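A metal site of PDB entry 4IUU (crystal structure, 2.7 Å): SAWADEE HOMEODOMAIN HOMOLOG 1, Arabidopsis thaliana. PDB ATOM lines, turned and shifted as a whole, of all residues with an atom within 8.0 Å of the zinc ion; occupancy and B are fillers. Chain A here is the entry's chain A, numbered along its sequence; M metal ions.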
ATOM      1  N   GLU A  64      17.846 -12.652 -29.101  1.00  0.00           N
ATOM      2  CA  GLU A  64      17.619 -11.313 -29.631  1.00  0.00           C
ATOM      3  C   GLU A  64      18.542 -10.284 -28.974  1.00  0.00           C
ATOM      4  O   GLU A  64      18.868 -10.407 -27.793  1.00  0.00           O
ATOM      5  CB  GLU A  64      16.167 -10.896 -29.413  1.00  0.00           C
ATOM      6  CG  GLU A  64      15.409 -10.574 -30.694  1.00  0.00           C
ATOM      7  CD  GLU A  64      13.926 -10.350 -30.458  1.00  0.00           C
ATOM      8  OE1 GLU A  64      13.424 -10.808 -29.413  1.00  0.00           O
ATOM      9  OE2 GLU A  64      13.274  -9.720 -31.314  1.00  0.00           O
ATOM     10  N   PRO A  65      18.951  -9.283 -29.741  1.00  0.00           N
ATOM     11  CA  PRO A  65      19.841  -8.237 -29.224  1.00  0.00           C
ATOM     12  C   PRO A  65      19.379  -7.670 -27.875  1.00  0.00           C
ATOM     13  O   PRO A  65      20.202  -7.508 -26.978  1.00  0.00           O
ATOM     14  CB  PRO A  65      19.770  -7.155 -30.300  1.00  0.00           C
ATOM     15  CG  PRO A  65      19.518  -7.909 -31.551  1.00  0.00           C
ATOM     16  CD  PRO A  65      18.657  -9.085 -31.173  1.00  0.00           C
ATOM     17  N   SER A  66      18.090  -7.376 -27.752  1.00  0.00           N
ATOM     18  CA  SER A  66      17.551  -6.772 -26.537  1.00  0.00           C
ATOM     19  C   SER A  66      17.551  -7.712 -25.329  1.00  0.00           C
ATOM     20  O   SER A  66      17.225  -7.289 -24.226  1.00  0.00           O
ATOM     21  CB  SER A  66      16.124  -6.229 -26.774  1.00  0.00           C
ATOM     22  OG  SER A  66      15.242  -7.260 -27.200  1.00  0.00           O
ATOM     23  N   GLU A  67      17.907  -8.966 -25.550  1.00  0.00           N
ATOM     24  CA  GLU A  67      17.991  -9.939 -24.451  1.00  0.00           C
ATOM     25  C   GLU A  67      19.365 -10.617 -24.329  1.00  0.00           C
ATOM     26  O   GLU A  67      19.488 -11.663 -23.693  1.00  0.00           O
ATOM     27  CB  GLU A  67      16.888 -10.992 -24.556  1.00  0.00           C
ATOM     28  CG  GLU A  67      16.770 -11.617 -25.930  1.00  0.00           C
ATOM     29  CD  GLU A  67      16.064 -12.961 -25.900  1.00  0.00           C
ATOM     30  OE1 GLU A  67      15.680 -13.411 -24.799  1.00  0.00           O
ATOM     31  OE2 GLU A  67      15.906 -13.574 -26.976  1.00  0.00           O
ATOM     32  N   CYS A  68      20.373 -10.016 -24.933  1.00  0.00           N
ATOM     33  CA  CYS A  68      21.719 -10.576 -24.932  1.00  0.00           C
ATOM     34  C   CYS A  68      22.300 -10.658 -23.522  1.00  0.00           C
ATOM     35  O   CYS A  68      23.362 -11.245 -23.310  1.00  0.00           O
ATOM     36  CB  CYS A  68      22.652  -9.741 -25.809  1.00  0.00           C
ATOM     37  SG  CYS A  68      23.063  -8.144 -25.067  1.00  0.00           S
ATOM     38  N   GLY A  69      21.602 -10.062 -22.562  1.00  0.00           N
ATOM     39  CA  GLY A  69      22.061 -10.043 -21.192  1.00  0.00           C
ATOM     40  C   GLY A  69      21.810 -11.360 -20.480  1.00  0.00           C
ATOM     41  O   GLY A  69      22.384 -11.622 -19.416  1.00  0.00           O
ATOM     42  N   ILE A  97      32.843 -12.361 -21.764  1.00  0.00           N
ATOM     43  CA  ILE A  97      31.938 -11.519 -22.543  1.00  0.00           C
ATOM     44  C   ILE A  97      32.366 -10.060 -22.544  1.00  0.00           C
ATOM     45  O   ILE A  97      32.607  -9.455 -21.490  1.00  0.00           O
ATOM     46  CB  ILE A  97      30.499 -11.601 -22.008  1.00  0.00           C
ATOM     47  CG1 ILE A  97      30.071 -13.051 -21.813  1.00  0.00           C
ATOM     48  CG2 ILE A  97      29.540 -10.881 -22.955  1.00  0.00           C
ATOM     49  CD1 ILE A  97      28.710 -13.208 -21.178  1.00  0.00           C
ATOM     50  N   LYS A  98      32.446  -9.479 -23.743  1.00  0.00           N
ATOM     51  CA  LYS A  98      32.756  -8.073 -23.911  1.00  0.00           C
ATOM     52  C   LYS A  98      31.495  -7.309 -24.296  1.00  0.00           C
ATOM     53  O   LYS A  98      31.080  -7.329 -25.445  1.00  0.00           O
ATOM     54  CB  LYS A  98      33.832  -7.875 -24.976  1.00  0.00           C
ATOM     55  CG  LYS A  98      35.250  -8.112 -24.487  1.00  0.00           C
ATOM     56  CD  LYS A  98      36.066  -8.873 -25.508  1.00  0.00           C
ATOM     57  CE  LYS A  98      37.555  -8.651 -25.307  1.00  0.00           C
ATOM     58  NZ  LYS A  98      37.901  -8.538 -23.867  1.00  0.00           N
ATOM     59  N   ARG A  99      30.887  -6.642 -23.318  1.00  0.00           N
ATOM     60  CA  ARG A  99      29.625  -5.948 -23.536  1.00  0.00           C
ATOM     61  C   ARG A  99      29.816  -4.685 -24.370  1.00  0.00           C
ATOM     62  O   ARG A  99      30.651  -3.839 -24.049  1.00  0.00           O
ATOM     63  CB  ARG A  99      28.951  -5.624 -22.197  1.00  0.00           C
ATOM     64  CG  ARG A  99      28.491  -6.856 -21.443  1.00  0.00           C
ATOM     65  CD  ARG A  99      27.489  -7.645 -22.276  1.00  0.00           C
ATOM     66  NE  ARG A  99      27.091  -8.890 -21.627  1.00  0.00           N
ATOM     67  CZ  ARG A  99      26.138  -9.700 -22.089  1.00  0.00           C
ATOM     68  NH1 ARG A  99      25.482  -9.376 -23.191  1.00  0.00           N
ATOM     69  NH2 ARG A  99      25.850 -10.813 -21.443  1.00  0.00           N
ATOM     70  N   GLY A 100      29.038  -4.566 -25.436  1.00  0.00           N
ATOM     71  CA  GLY A 100      29.128  -3.423 -26.317  1.00  0.00           C
ATOM     72  C   GLY A 100      28.004  -2.430 -26.109  1.00  0.00           C
ATOM     73  O   GLY A 100      27.105  -2.649 -25.309  1.00  0.00           O
ATOM     74  N   ILE A 101      28.072  -1.325 -26.850  1.00  0.00           N
ATOM     75  CA  ILE A 101      27.040  -0.302 -26.797  1.00  0.00           C
ATOM     76  C   ILE A 101      26.120  -0.467 -28.000  1.00  0.00           C
ATOM     77  O   ILE A 101      26.528  -0.236 -29.138  1.00  0.00           O
ATOM     78  CB  ILE A 101      27.651   1.112 -26.827  1.00  0.00           C
ATOM     79  CG1 ILE A 101      28.557   1.327 -25.616  1.00  0.00           C
ATOM     80  CG2 ILE A 101      26.551   2.160 -26.874  1.00  0.00           C
ATOM     81  CD1 ILE A 101      29.404   2.577 -25.705  1.00  0.00           C
ATOM     82  N   HIS A 102      24.881  -0.862 -27.740  1.00  0.00           N
ATOM     83  CA  HIS A 102      23.924  -1.055 -28.819  1.00  0.00           C
ATOM     84  C   HIS A 102      22.485  -1.046 -28.311  1.00  0.00           C
ATOM     85  O   HIS A 102      22.228  -1.118 -27.116  1.00  0.00           O
ATOM     86  CB  HIS A 102      24.212  -2.351 -29.563  1.00  0.00           C
ATOM     87  CG  HIS A 102      23.918  -3.583 -28.766  1.00  0.00           C
ATOM     88  ND1 HIS A 102      22.647  -3.962 -28.421  1.00  0.00           N
ATOM     89  CD2 HIS A 102      24.748  -4.512 -28.236  1.00  0.00           C
ATOM     90  CE1 HIS A 102      22.698  -5.084 -27.710  1.00  0.00           C
ATOM     91  NE2 HIS A 102      23.966  -5.432 -27.586  1.00  0.00           N
ATOM     92  N   ASP A 103      21.553  -0.966 -29.256  1.00  0.00           N
ATOM     93  CA  ASP A 103      20.132  -0.976 -28.935  1.00  0.00           C
ATOM     94  C   ASP A 103      19.528  -2.367 -29.116  1.00  0.00           C
ATOM     95  O   ASP A 103      20.157  -3.377 -28.818  1.00  0.00           O
ATOM     96  CB  ASP A 103      19.381   0.034 -29.805  1.00  0.00           C
ATOM     97  CG  ASP A 103      19.564  -0.220 -31.286  1.00  0.00           C
ATOM     98  OD1 ASP A 103      19.840  -1.386 -31.661  1.00  0.00           O
ATOM     99  OD2 ASP A 103      19.428   0.725 -32.084  1.00  0.00           O
ATOM    100  N   ARG A 106      20.659  -4.496 -33.119  1.00  0.00           N
ATOM    101  CA  ARG A 106      21.768  -5.431 -33.287  1.00  0.00           C
ATOM    102  C   ARG A 106      22.693  -5.456 -32.072  1.00  0.00           C
ATOM    103  O   ARG A 106      22.923  -4.438 -31.426  1.00  0.00           O
ATOM    104  CB  ARG A 106      22.561  -5.096 -34.559  1.00  0.00           C
ATOM    105  CG  ARG A 106      23.604  -6.142 -34.921  1.00  0.00           C
ATOM    106  CD  ARG A 106      23.988  -6.052 -36.388  1.00  0.00           C
ATOM    107  NE  ARG A 106      24.980  -7.058 -36.756  1.00  0.00           N
ATOM    108  CZ  ARG A 106      24.685  -8.232 -37.319  1.00  0.00           C
ATOM    109  NH1 ARG A 106      25.653  -9.082 -37.622  1.00  0.00           N
ATOM    110  NH2 ARG A 106      23.422  -8.547 -37.579  1.00  0.00           N
ATOM    111  N   CYS A 107      23.223  -6.638 -31.771  1.00  0.00           N
ATOM    112  CA  CYS A 107      24.096  -6.820 -30.619  1.00  0.00           C
ATOM    113  C   CYS A 107      25.558  -6.934 -31.050  1.00  0.00           C
ATOM    114  O   CYS A 107      25.928  -7.870 -31.749  1.00  0.00           O
ATOM    115  CB  CYS A 107      23.689  -8.063 -29.834  1.00  0.00           C
ATOM    116  SG  CYS A 107      24.963  -8.718 -28.729  1.00  0.00           S
ATOM    117  N   ASN A 108      26.374  -5.974 -30.621  1.00  0.00           N
ATOM    118  CA  ASN A 108      27.778  -5.962 -30.981  1.00  0.00           C
ATOM    119  C   ASN A 108      28.695  -6.493 -29.866  1.00  0.00           C
ATOM    120  O   ASN A 108      29.912  -6.340 -29.934  1.00  0.00           O
ATOM    121  CB  ASN A 108      28.207  -4.549 -31.403  1.00  0.00           C
ATOM    122  CG  ASN A 108      28.026  -3.523 -30.302  1.00  0.00           C
ATOM    123  OD1 ASN A 108      27.468  -3.822 -29.248  1.00  0.00           O
ATOM    124  ND2 ASN A 108      28.484  -2.309 -30.554  1.00  0.00           N
ATOM    125  N   CYS A 109      28.089  -7.120 -28.861  1.00  0.00           N
ATOM    126  CA  CYS A 109      28.863  -7.789 -27.821  1.00  0.00           C
ATOM    127  C   CYS A 109      29.681  -8.913 -28.435  1.00  0.00           C
ATOM    128  O   CYS A 109      29.286  -9.493 -29.451  1.00  0.00           O
ATOM    129  CB  CYS A 109      27.930  -8.355 -26.746  1.00  0.00           C
ATOM    130  SG  CYS A 109      27.132  -7.104 -25.708  1.00  0.00           S
ATOM    131  N   VAL A 110      30.815  -9.221 -27.824  1.00  0.00           N
ATOM    132  CA  VAL A 110      31.655 -10.314 -28.299  1.00  0.00           C
ATOM    133  C   VAL A 110      31.706 -11.424 -27.254  1.00  0.00           C
ATOM    134  O   VAL A 110      31.975 -11.166 -26.082  1.00  0.00           O
ATOM    135  CB  VAL A 110      33.080  -9.843 -28.622  1.00  0.00           C
ATOM    136  CG1 VAL A 110      33.925 -11.014 -29.110  1.00  0.00           C
ATOM    137  CG2 VAL A 110      33.051  -8.742 -29.669  1.00  0.00           C
ATOM    138  N   PHE A 111      31.460 -12.645 -27.694  1.00  0.00           N
ATOM    139  CA  PHE A 111      31.439 -13.798 -26.797  1.00  0.00           C
ATOM    140  C   PHE A 111      32.604 -14.736 -27.083  1.00  0.00           C
ATOM    141  O   PHE A 111      32.684 -15.324 -28.163  1.00  0.00           O
ATOM    142  CB  PHE A 111      30.120 -14.561 -26.946  1.00  0.00           C
ATOM    143  CG  PHE A 111      28.902 -13.721 -26.719  1.00  0.00           C
ATOM    144  CD1 PHE A 111      28.214 -13.780 -25.517  1.00  0.00           C
ATOM    145  CD2 PHE A 111      28.431 -12.871 -27.706  1.00  0.00           C
ATOM    146  CE1 PHE A 111      27.086 -12.998 -25.302  1.00  0.00           C
ATOM    147  CE2 PHE A 111      27.307 -12.098 -27.501  1.00  0.00           C
ATOM    148  CZ  PHE A 111      26.640 -12.157 -26.301  1.00  0.00           C
ATOM    149  N   LEU A 126      26.527 -12.411 -31.353  1.00  0.00           N
ATOM    150  CA  LEU A 126      25.233 -12.992 -31.008  1.00  0.00           C
ATOM    151  C   LEU A 126      24.563 -13.665 -32.200  1.00  0.00           C
ATOM    152  O   LEU A 126      23.862 -14.667 -32.040  1.00  0.00           O
ATOM    153  CB  LEU A 126      24.309 -11.917 -30.427  1.00  0.00           C
ATOM    154  CG  LEU A 126      23.043 -12.436 -29.735  1.00  0.00           C
ATOM    155  CD1 LEU A 126      23.403 -13.078 -28.402  1.00  0.00           C
ATOM    156  CD2 LEU A 126      22.032 -11.321 -29.540  1.00  0.00           C
HETATM  157 ZN    ZN M   1      24.764  -7.238 -26.630  1.00  0.00          ZN
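N of Gly 100 lies close to SG of Cys 109 (3.2 Å).
The side-chain sulfur of Cys 68 sits close to the backbone carbonyl oxygen of Pro 65 (3.5 Å).
A ring nitrogen (ND1) of His 102 lies close to the backbone carbonyl oxygen (O) of Arg 106 (3.1 Å).
The guanidinium group (NH1) of Arg 99 lies close to the side-chain sulfur (SG) of Cys 109 (3.8 Å).
The backbone carbonyl oxygen of Cys 68 lies within hydrogen-bond range of the guanidinium group of Arg 99 (2.8 Å).
The zinc ion is bound by NE2 of His 102 (2.2 Å), SG of Cys 68 (2.5 Å), SG of Cys 109 (2.5 Å) and SG of Cys 107 (2.6 Å).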
